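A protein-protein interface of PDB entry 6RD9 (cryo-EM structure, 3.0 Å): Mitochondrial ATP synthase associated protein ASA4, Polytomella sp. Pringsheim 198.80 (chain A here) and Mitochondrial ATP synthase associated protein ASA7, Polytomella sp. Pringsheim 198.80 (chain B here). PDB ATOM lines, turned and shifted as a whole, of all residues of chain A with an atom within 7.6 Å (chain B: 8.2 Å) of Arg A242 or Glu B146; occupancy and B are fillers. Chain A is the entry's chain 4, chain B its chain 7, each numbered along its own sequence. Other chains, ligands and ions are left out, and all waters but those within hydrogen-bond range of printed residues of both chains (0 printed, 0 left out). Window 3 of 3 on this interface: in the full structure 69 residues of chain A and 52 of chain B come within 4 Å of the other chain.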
ATOM      1  N   LEU A 230       4.887  21.559 -19.540  1.00  0.00           N
ATOM      2  CA  LEU A 230       5.023  22.943 -19.955  1.00  0.00           C
ATOM      3  C   LEU A 230       6.431  23.457 -19.726  1.00  0.00           C
ATOM      4  O   LEU A 230       7.005  24.091 -20.613  1.00  0.00           O
ATOM      5  CB  LEU A 230       4.025  23.806 -19.206  1.00  0.00           C
ATOM      6  CG  LEU A 230       4.031  25.245 -19.640  1.00  0.00           C
ATOM      7  CD1 LEU A 230       3.338  25.334 -20.937  1.00  0.00           C
ATOM      8  CD2 LEU A 230       3.343  26.043 -18.633  1.00  0.00           C
ATOM      9  N   HIS A 233       8.669  22.416 -22.227  1.00  0.00           N
ATOM     10  CA  HIS A 233       8.332  23.057 -23.488  1.00  0.00           C
ATOM     11  C   HIS A 233       8.678  24.530 -23.485  1.00  0.00           C
ATOM     12  O   HIS A 233       9.022  25.074 -24.531  1.00  0.00           O
ATOM     13  CB  HIS A 233       6.844  22.817 -23.761  1.00  0.00           C
ATOM     14  CG  HIS A 233       6.193  23.781 -24.701  1.00  0.00           C
ATOM     15  ND1 HIS A 233       5.674  24.985 -24.285  1.00  0.00           N
ATOM     16  CD2 HIS A 233       5.866  23.665 -26.004  1.00  0.00           C
ATOM     17  CE1 HIS A 233       5.117  25.600 -25.308  1.00  0.00           C
ATOM     18  NE2 HIS A 233       5.217  24.819 -26.363  1.00  0.00           N
ATOM     19  N   LEU A 234       8.624  25.192 -22.333  1.00  0.00           N
ATOM     20  CA  LEU A 234       9.028  26.588 -22.255  1.00  0.00           C
ATOM     21  C   LEU A 234      10.530  26.773 -22.350  1.00  0.00           C
ATOM     22  O   LEU A 234      10.987  27.902 -22.527  1.00  0.00           O
ATOM     23  CB  LEU A 234       8.541  27.215 -20.961  1.00  0.00           C
ATOM     24  CG  LEU A 234       7.056  27.441 -20.825  1.00  0.00           C
ATOM     25  CD1 LEU A 234       6.802  28.134 -19.550  1.00  0.00           C
ATOM     26  CD2 LEU A 234       6.567  28.267 -21.940  1.00  0.00           C
ATOM     27  N   LYS A 236      12.303  25.378 -24.693  1.00  0.00           N
ATOM     28  CA  LYS A 236      12.655  25.177 -26.081  1.00  0.00           C
ATOM     29  C   LYS A 236      12.584  26.489 -26.844  1.00  0.00           C
ATOM     30  O   LYS A 236      11.812  27.378 -26.491  1.00  0.00           O
ATOM     31  CB  LYS A 236      11.709  24.182 -26.746  1.00  0.00           C
ATOM     32  CG  LYS A 236      11.723  22.807 -26.177  1.00  0.00           C
ATOM     33  CD  LYS A 236      10.832  21.915 -26.998  1.00  0.00           C
ATOM     34  CE  LYS A 236      10.203  20.817 -26.174  1.00  0.00           C
ATOM     35  NZ  LYS A 236      11.207  19.943 -25.557  1.00  0.00           N
ATOM     36  N   PRO A 237      13.379  26.660 -27.887  1.00  0.00           N
ATOM     37  CA  PRO A 237      13.130  27.756 -28.815  1.00  0.00           C
ATOM     38  C   PRO A 237      11.914  27.461 -29.667  1.00  0.00           C
ATOM     39  O   PRO A 237      11.546  26.312 -29.886  1.00  0.00           O
ATOM     40  CB  PRO A 237      14.398  27.800 -29.661  1.00  0.00           C
ATOM     41  CG  PRO A 237      14.964  26.465 -29.534  1.00  0.00           C
ATOM     42  CD  PRO A 237      14.665  26.012 -28.160  1.00  0.00           C
ATOM     43  N   VAL A 238      11.315  28.534 -30.180  1.00  0.00           N
ATOM     44  CA  VAL A 238      10.015  28.464 -30.838  1.00  0.00           C
ATOM     45  C   VAL A 238      10.088  27.703 -32.144  1.00  0.00           C
ATOM     46  O   VAL A 238       9.118  27.066 -32.551  1.00  0.00           O
ATOM     47  CB  VAL A 238       9.494  29.883 -31.065  1.00  0.00           C
ATOM     48  CG1 VAL A 238       8.069  29.874 -31.387  1.00  0.00           C
ATOM     49  CG2 VAL A 238       9.725  30.667 -29.860  1.00  0.00           C
ATOM     50  N   ALA A 239      11.227  27.747 -32.825  1.00  0.00           N
ATOM     51  CA  ALA A 239      11.352  27.015 -34.072  1.00  0.00           C
ATOM     52  C   ALA A 239      11.382  25.519 -33.836  1.00  0.00           C
ATOM     53  O   ALA A 239      10.942  24.752 -34.694  1.00  0.00           O
ATOM     54  CB  ALA A 239      12.605  27.456 -34.809  1.00  0.00           C
ATOM     55  N   GLN A 240      11.885  25.091 -32.683  1.00  0.00           N
ATOM     56  CA  GLN A 240      11.863  23.676 -32.346  1.00  0.00           C
ATOM     57  C   GLN A 240      10.455  23.221 -32.036  1.00  0.00           C
ATOM     58  O   GLN A 240      10.054  22.123 -32.427  1.00  0.00           O
ATOM     59  CB  GLN A 240      12.775  23.413 -31.158  1.00  0.00           C
ATOM     60  CG  GLN A 240      12.840  21.981 -30.759  1.00  0.00           C
ATOM     61  CD  GLN A 240      13.710  21.760 -29.559  1.00  0.00           C
ATOM     62  OE1 GLN A 240      13.653  20.710 -28.926  1.00  0.00           O
ATOM     63  NE2 GLN A 240      14.528  22.748 -29.234  1.00  0.00           N
ATOM     64  N   ILE A 241       9.686  24.072 -31.358  1.00  0.00           N
ATOM     65  CA  ILE A 241       8.349  23.721 -30.897  1.00  0.00           C
ATOM     66  C   ILE A 241       7.411  23.527 -32.069  1.00  0.00           C
ATOM     67  O   ILE A 241       6.687  22.533 -32.135  1.00  0.00           O
ATOM     68  CB  ILE A 241       7.829  24.810 -29.951  1.00  0.00           C
ATOM     69  CG1 ILE A 241       8.531  24.746 -28.619  1.00  0.00           C
ATOM     70  CG2 ILE A 241       6.373  24.692 -29.747  1.00  0.00           C
ATOM     71  CD1 ILE A 241       8.138  25.852 -27.746  1.00  0.00           C
ATOM     72  N   ARG A 242       7.437  24.450 -33.027  1.00  0.00           N
ATOM     73  CA  ARG A 242       6.492  24.414 -34.131  1.00  0.00           C
ATOM     74  C   ARG A 242       6.735  23.236 -35.051  1.00  0.00           C
ATOM     75  O   ARG A 242       5.797  22.742 -35.672  1.00  0.00           O
ATOM     76  CB  ARG A 242       6.571  25.697 -34.936  1.00  0.00           C
ATOM     77  CG  ARG A 242       6.301  26.922 -34.152  1.00  0.00           C
ATOM     78  CD  ARG A 242       5.708  27.965 -35.024  1.00  0.00           C
ATOM     79  NE  ARG A 242       5.630  29.242 -34.347  1.00  0.00           N
ATOM     80  CZ  ARG A 242       6.451  30.247 -34.586  1.00  0.00           C
ATOM     81  NH1 ARG A 242       7.409  30.111 -35.488  1.00  0.00           N
ATOM     82  NH2 ARG A 242       6.314  31.385 -33.930  1.00  0.00           N
ATOM     83  N   LYS A 243       7.971  22.767 -35.149  1.00  0.00           N
ATOM     84  CA  LYS A 243       8.255  21.620 -35.989  1.00  0.00           C
ATOM     85  C   LYS A 243       8.246  20.310 -35.225  1.00  0.00           C
ATOM     86  O   LYS A 243       8.125  19.260 -35.852  1.00  0.00           O
ATOM     87  CB  LYS A 243       9.594  21.797 -36.700  1.00  0.00           C
ATOM     88  CG  LYS A 243      10.800  21.620 -35.820  1.00  0.00           C
ATOM     89  CD  LYS A 243      12.038  21.368 -36.647  1.00  0.00           C
ATOM     90  CE  LYS A 243      11.876  20.117 -37.479  1.00  0.00           C
ATOM     91  NZ  LYS A 243      11.491  18.965 -36.624  1.00  0.00           N
ATOM     92  N   GLU A 244       8.379  20.336 -33.900  1.00  0.00           N
ATOM     93  CA  GLU A 244       8.113  19.133 -33.120  1.00  0.00           C
ATOM     94  C   GLU A 244       6.634  18.807 -33.134  1.00  0.00           C
ATOM     95  O   GLU A 244       6.249  17.638 -33.148  1.00  0.00           O
ATOM     96  CB  GLU A 244       8.570  19.309 -31.682  1.00  0.00           C
ATOM     97  CG  GLU A 244       9.978  18.905 -31.402  1.00  0.00           C
ATOM     98  CD  GLU A 244      10.266  18.879 -29.917  1.00  0.00           C
ATOM     99  OE1 GLU A 244       9.604  19.630 -29.173  1.00  0.00           O
ATOM    100  OE2 GLU A 244      11.143  18.099 -29.491  1.00  0.00           O
ATOM    101  N   GLN A 245       5.797  19.834 -33.114  1.00  0.00           N
ATOM    102  CA  GLN A 245       4.362  19.640 -33.081  1.00  0.00           C
ATOM    103  C   GLN A 245       3.781  19.385 -34.453  1.00  0.00           C
ATOM    104  O   GLN A 245       2.804  18.648 -34.568  1.00  0.00           O
ATOM    105  CB  GLN A 245       3.694  20.855 -32.474  1.00  0.00           C
ATOM    106  CG  GLN A 245       3.972  21.026 -31.027  1.00  0.00           C
ATOM    107  CD  GLN A 245       3.179  22.141 -30.469  1.00  0.00           C
ATOM    108  OE1 GLN A 245       2.668  22.967 -31.210  1.00  0.00           O
ATOM    109  NE2 GLN A 245       3.060  22.187 -29.158  1.00  0.00           N
ATOM    110  N   ALA A 246       4.329  20.002 -35.493  1.00  0.00           N
ATOM    111  CA  ALA A 246       3.877  19.696 -36.839  1.00  0.00           C
ATOM    112  C   ALA A 246       4.325  18.325 -37.293  1.00  0.00           C
ATOM    113  O   ALA A 246       3.644  17.710 -38.115  1.00  0.00           O
ATOM    114  CB  ALA A 246       4.381  20.735 -37.827  1.00  0.00           C
ATOM    115  N   SER A 247       5.458  17.841 -36.787  1.00  0.00           N
ATOM    116  CA  SER A 247       5.847  16.461 -37.035  1.00  0.00           C
ATOM    117  C   SER A 247       4.922  15.496 -36.323  1.00  0.00           C
ATOM    118  O   SER A 247       4.581  14.443 -36.866  1.00  0.00           O
ATOM    119  CB  SER A 247       7.278  16.225 -36.578  1.00  0.00           C
ATOM    120  OG  SER A 247       7.594  14.850 -36.641  1.00  0.00           O
ATOM    121  N   ALA A 248       4.515  15.831 -35.103  1.00  0.00           N
ATOM    122  CA  ALA A 248       3.631  14.953 -34.356  1.00  0.00           C
ATOM    123  C   ALA A 248       2.203  15.029 -34.861  1.00  0.00           C
ATOM    124  O   ALA A 248       1.470  14.048 -34.767  1.00  0.00           O
ATOM    125  CB  ALA A 248       3.680  15.292 -32.872  1.00  0.00           C
ATOM    126  N   LEU B  94      -2.802  27.337 -20.087  1.00  0.00           N
ATOM    127  CA  LEU B  94      -2.876  28.775 -20.289  1.00  0.00           C
ATOM    128  C   LEU B  94      -2.784  29.511 -18.973  1.00  0.00           C
ATOM    129  O   LEU B  94      -2.294  30.632 -18.919  1.00  0.00           O
ATOM    130  CB  LEU B  94      -4.167  29.136 -20.995  1.00  0.00           C
ATOM    131  CG  LEU B  94      -4.283  30.529 -21.568  1.00  0.00           C
ATOM    132  CD1 LEU B  94      -3.554  30.586 -22.846  1.00  0.00           C
ATOM    133  CD2 LEU B  94      -5.708  30.845 -21.782  1.00  0.00           C
ATOM    134  N   SER B  97       0.994  29.232 -18.106  1.00  0.00           N
ATOM    135  CA  SER B  97       1.765  30.173 -18.907  1.00  0.00           C
ATOM    136  C   SER B  97       1.615  31.587 -18.419  1.00  0.00           C
ATOM    137  O   SER B  97       2.494  32.406 -18.652  1.00  0.00           O
ATOM    138  CB  SER B  97       1.347  30.139 -20.359  1.00  0.00           C
ATOM    139  OG  SER B  97       1.824  28.988 -20.983  1.00  0.00           O
ATOM    140  N   TYR B 101       4.665  34.098 -17.664  1.00  0.00           N
ATOM    141  CA  TYR B 101       4.654  35.409 -18.277  1.00  0.00           C
ATOM    142  C   TYR B 101       4.707  36.514 -17.240  1.00  0.00           C
ATOM    143  O   TYR B 101       5.150  37.616 -17.546  1.00  0.00           O
ATOM    144  CB  TYR B 101       3.394  35.515 -19.118  1.00  0.00           C
ATOM    145  CG  TYR B 101       3.120  36.791 -19.839  1.00  0.00           C
ATOM    146  CD1 TYR B 101       3.454  36.935 -21.161  1.00  0.00           C
ATOM    147  CD2 TYR B 101       2.446  37.822 -19.223  1.00  0.00           C
ATOM    148  CE1 TYR B 101       3.167  38.076 -21.815  1.00  0.00           C
ATOM    149  CE2 TYR B 101       2.188  38.961 -19.868  1.00  0.00           C
ATOM    150  CZ  TYR B 101       2.538  39.077 -21.158  1.00  0.00           C
ATOM    151  OH  TYR B 101       2.238  40.231 -21.787  1.00  0.00           O
ATOM    152  N   LEU B 140      13.032  33.368 -24.325  1.00  0.00           N
ATOM    153  CA  LEU B 140      12.051  32.979 -23.327  1.00  0.00           C
ATOM    154  C   LEU B 140      10.712  33.628 -23.597  1.00  0.00           C
ATOM    155  O   LEU B 140       9.674  33.008 -23.397  1.00  0.00           O
ATOM    156  CB  LEU B 140      12.522  33.370 -21.936  1.00  0.00           C
ATOM    157  CG  LEU B 140      13.880  32.907 -21.466  1.00  0.00           C
ATOM    158  CD1 LEU B 140      14.145  33.449 -20.102  1.00  0.00           C
ATOM    159  CD2 LEU B 140      13.924  31.431 -21.483  1.00  0.00           C
ATOM    160  N   TYR B 141      10.712  34.872 -24.040  1.00  0.00           N
ATOM    161  CA  TYR B 141       9.463  35.580 -24.238  1.00  0.00           C
ATOM    162  C   TYR B 141       8.749  35.156 -25.501  1.00  0.00           C
ATOM    163  O   TYR B 141       7.524  35.185 -25.543  1.00  0.00           O
ATOM    164  CB  TYR B 141       9.717  37.070 -24.275  1.00  0.00           C
ATOM    165  CG  TYR B 141       8.485  37.895 -24.295  1.00  0.00           C
ATOM    166  CD1 TYR B 141       7.750  38.093 -23.158  1.00  0.00           C
ATOM    167  CD2 TYR B 141       8.061  38.493 -25.455  1.00  0.00           C
ATOM    168  CE1 TYR B 141       6.634  38.851 -23.180  1.00  0.00           C
ATOM    169  CE2 TYR B 141       6.943  39.253 -25.478  1.00  0.00           C
ATOM    170  CZ  TYR B 141       6.239  39.425 -24.344  1.00  0.00           C
ATOM    171  OH  TYR B 141       5.115  40.185 -24.385  1.00  0.00           O
ATOM    172  N   GLU B 142       9.465  34.774 -26.542  1.00  0.00           N
ATOM    173  CA  GLU B 142       8.779  34.357 -27.750  1.00  0.00           C
ATOM    174  C   GLU B 142       8.226  32.957 -27.650  1.00  0.00           C
ATOM    175  O   GLU B 142       7.433  32.570 -28.501  1.00  0.00           O
ATOM    176  CB  GLU B 142       9.698  34.465 -28.963  1.00  0.00           C
ATOM    177  CG  GLU B 142      10.014  35.901 -29.353  1.00  0.00           C
ATOM    178  CD  GLU B 142      10.733  36.020 -30.677  1.00  0.00           C
ATOM    179  OE1 GLU B 142      11.611  35.173 -30.957  1.00  0.00           O
ATOM    180  OE2 GLU B 142      10.431  36.973 -31.430  1.00  0.00           O
ATOM    181  N   THR B 143       8.629  32.180 -26.655  1.00  0.00           N
ATOM    182  CA  THR B 143       8.047  30.867 -26.467  1.00  0.00           C
ATOM    183  C   THR B 143       6.991  30.827 -25.382  1.00  0.00           C
ATOM    184  O   THR B 143       6.187  29.902 -25.376  1.00  0.00           O
ATOM    185  CB  THR B 143       9.117  29.817 -26.157  1.00  0.00           C
ATOM    186  OG1 THR B 143       8.480  28.558 -26.008  1.00  0.00           O
ATOM    187  CG2 THR B 143       9.799  30.096 -24.898  1.00  0.00           C
ATOM    188  N   VAL B 144       6.946  31.795 -24.474  1.00  0.00           N
ATOM    189  CA  VAL B 144       5.880  31.784 -23.492  1.00  0.00           C
ATOM    190  C   VAL B 144       4.628  32.403 -24.080  1.00  0.00           C
ATOM    191  O   VAL B 144       3.529  32.168 -23.567  1.00  0.00           O
ATOM    192  CB  VAL B 144       6.290  32.494 -22.193  1.00  0.00           C
ATOM    193  CG1 VAL B 144       6.137  33.954 -22.304  1.00  0.00           C
ATOM    194  CG2 VAL B 144       5.519  31.983 -21.034  1.00  0.00           C
ATOM    195  N   THR B 145       4.754  33.151 -25.167  1.00  0.00           N
ATOM    196  CA  THR B 145       3.622  33.726 -25.855  1.00  0.00           C
ATOM    197  C   THR B 145       3.250  32.920 -27.071  1.00  0.00           C
ATOM    198  O   THR B 145       2.432  33.358 -27.866  1.00  0.00           O
ATOM    199  CB  THR B 145       3.909  35.164 -26.230  1.00  0.00           C
ATOM    200  OG1 THR B 145       5.007  35.200 -27.128  1.00  0.00           O
ATOM    201  CG2 THR B 145       4.287  35.915 -25.022  1.00  0.00           C
ATOM    202  N   GLU B 146       3.813  31.736 -27.215  1.00  0.00           N
ATOM    203  CA  GLU B 146       3.386  30.783 -28.225  1.00  0.00           C
ATOM    204  C   GLU B 146       2.210  30.008 -27.643  1.00  0.00           C
ATOM    205  O   GLU B 146       2.323  28.862 -27.215  1.00  0.00           O
ATOM    206  CB  GLU B 146       4.548  29.882 -28.601  1.00  0.00           C
ATOM    207  CG  GLU B 146       4.324  28.946 -29.735  1.00  0.00           C
ATOM    208  CD  GLU B 146       4.179  29.634 -31.039  1.00  0.00           C
ATOM    209  OE1 GLU B 146       4.851  30.657 -31.239  1.00  0.00           O
ATOM    210  OE2 GLU B 146       3.402  29.159 -31.886  1.00  0.00           O
ATOM    211  N   PHE B 147       1.057  30.665 -27.601  1.00  0.00           N
ATOM    212  CA  PHE B 147      -0.127  30.068 -27.010  1.00  0.00           C
ATOM    213  C   PHE B 147      -0.844  29.124 -27.948  1.00  0.00           C
ATOM    214  O   PHE B 147      -1.751  28.425 -27.507  1.00  0.00           O
ATOM    215  CB  PHE B 147      -1.118  31.132 -26.583  1.00  0.00           C
ATOM    216  CG  PHE B 147      -0.574  32.132 -25.640  1.00  0.00           C
ATOM    217  CD1 PHE B 147      -0.127  31.766 -24.411  1.00  0.00           C
ATOM    218  CD2 PHE B 147      -0.549  33.454 -25.978  1.00  0.00           C
ATOM    219  CE1 PHE B 147       0.341  32.704 -23.549  1.00  0.00           C
ATOM    220  CE2 PHE B 147      -0.092  34.381 -25.118  1.00  0.00           C
ATOM    221  CZ  PHE B 147       0.360  34.007 -23.912  1.00  0.00           C
ATOM    222  N   ASP B 148      -0.490  29.088 -29.221  1.00  0.00           N
ATOM    223  CA  ASP B 148      -1.026  28.089 -30.125  1.00  0.00           C
ATOM    224  C   ASP B 148      -0.350  26.747 -29.965  1.00  0.00           C
ATOM    225  O   ASP B 148      -0.714  25.796 -30.654  1.00  0.00           O
ATOM    226  CB  ASP B 148      -0.886  28.543 -31.567  1.00  0.00           C
ATOM    227  CG  ASP B 148      -1.918  29.559 -31.959  1.00  0.00           C
ATOM    228  OD1 ASP B 148      -2.705  29.979 -31.092  1.00  0.00           O
ATOM    229  OD2 ASP B 148      -1.945  29.942 -33.145  1.00  0.00           O
ATOM    230  N   SER B 149       0.632  26.649 -29.088  1.00  0.00           N
ATOM    231  CA  SER B 149       1.253  25.385 -28.767  1.00  0.00           C
ATOM    232  C   SER B 149       0.687  24.750 -27.521  1.00  0.00           C
ATOM    233  O   SER B 149       1.048  23.618 -27.213  1.00  0.00           O
ATOM    234  CB  SER B 149       2.744  25.578 -28.599  1.00  0.00           C
ATOM    235  OG  SER B 149       3.305  25.869 -29.854  1.00  0.00           O
ATOM    236  N   LEU B 150      -0.170  25.449 -26.792  1.00  0.00           N
ATOM    237  CA  LEU B 150      -0.728  24.868 -25.589  1.00  0.00           C
ATOM    238  C   LEU B 150      -1.813  23.863 -25.895  1.00  0.00           C
ATOM    239  O   LEU B 150      -2.077  22.996 -25.069  1.00  0.00           O
ATOM    240  CB  LEU B 150      -1.275  25.954 -24.686  1.00  0.00           C
ATOM    241  CG  LEU B 150      -0.250  26.969 -24.244  1.00  0.00           C
ATOM    242  CD1 LEU B 150      -0.903  27.925 -23.350  1.00  0.00           C
ATOM    243  CD2 LEU B 150       0.840  26.292 -23.533  1.00  0.00           C
ATOM    244  N   SER B 151      -2.446  23.950 -27.048  1.00  0.00           N
ATOM    245  CA  SER B 151      -3.505  23.017 -27.370  1.00  0.00           C
ATOM    246  C   SER B 151      -2.987  21.665 -27.783  1.00  0.00           C
ATOM    247  O   SER B 151      -3.757  20.715 -27.791  1.00  0.00           O
ATOM    248  CB  SER B 151      -4.377  23.554 -28.484  1.00  0.00           C
ATOM    249  OG  SER B 151      -5.176  22.519 -29.002  1.00  0.00           O
ATOM    250  N   LEU B 153      -0.063  20.537 -26.282  1.00  0.00           N
ATOM    251  CA  LEU B 153       0.470  20.025 -25.034  1.00  0.00           C
ATOM    252  C   LEU B 153      -0.619  19.434 -24.177  1.00  0.00           C
ATOM    253  O   LEU B 153      -0.337  18.626 -23.295  1.00  0.00           O
ATOM    254  CB  LEU B 153       1.144  21.121 -24.236  1.00  0.00           C
ATOM    255  CG  LEU B 153       2.390  21.823 -24.684  1.00  0.00           C
ATOM    256  CD1 LEU B 153       2.723  22.729 -23.580  1.00  0.00           C
ATOM    257  CD2 LEU B 153       3.443  20.810 -24.864  1.00  0.00           C
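NH2 of Arg A242 is in salt-bridge range of OE1 of Glu B146.
The backbone carbonyl oxygen of Ser B149 lies within hydrogen-bond range of the side-chain amide nitrogen of Gln A245, 3.1 Å away.
Of the printed residues of chain B, Leu A230 touches Ser B97 (3.96 Å), Leu B150 (3.7 Å) and Leu B153 (3.8 Å).
Printed residues of chain B within 4 Å of Lys A236: Thr B143.
Arg A242 touches just one residue of chain B: Glu B146.
Glu B146 touches two residues of chain A.
Printed residues of chain A within 4 Å of Ser B149: His A233 (3.4 Å), Ile A241 (3.3 Å) and Gln A245 (3.1 Å).
Printed residues of chain A within 4 Å of Leu B153: Leu A230 and His A233.
The nearest residue of chain B that does not touch Arg A242 is Ser B149 (5.3 Å).
The nearest printed residue of chain A that does not touch Glu B146 is His A233 (4.7 Å).
Among the printed residues, pairs that only touch across the chains: Ile A241 with Thr B143, Val A238 with Glu B142, Ile A241 with Ser B149, Val A238 with Glu B146, His A233 with Ser B149, Leu A234 with Thr B143, Lys A236 with Thr B143, Val A238 with Thr B143, Leu A230 with Leu B150, Leu A230 with Leu B153, His A233 with Leu B153, His A233 with Thr B143, Leu A234 with Val B144 and Leu A230 with Ser B97.
Of the 16 printed residues of chain A, 8 touch a printed residue of chain B.
Of the 16 printed residues of chain B, 8 touch a printed residue of chain A.
Hydrophobic or aromatic side chains of chain B that line the printed part of chain A: Val B144, Leu B150 and Leu B153.
NZ of Lys A236 is in salt-bridge range of OE1 of Glu A244 (3.97 Å).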
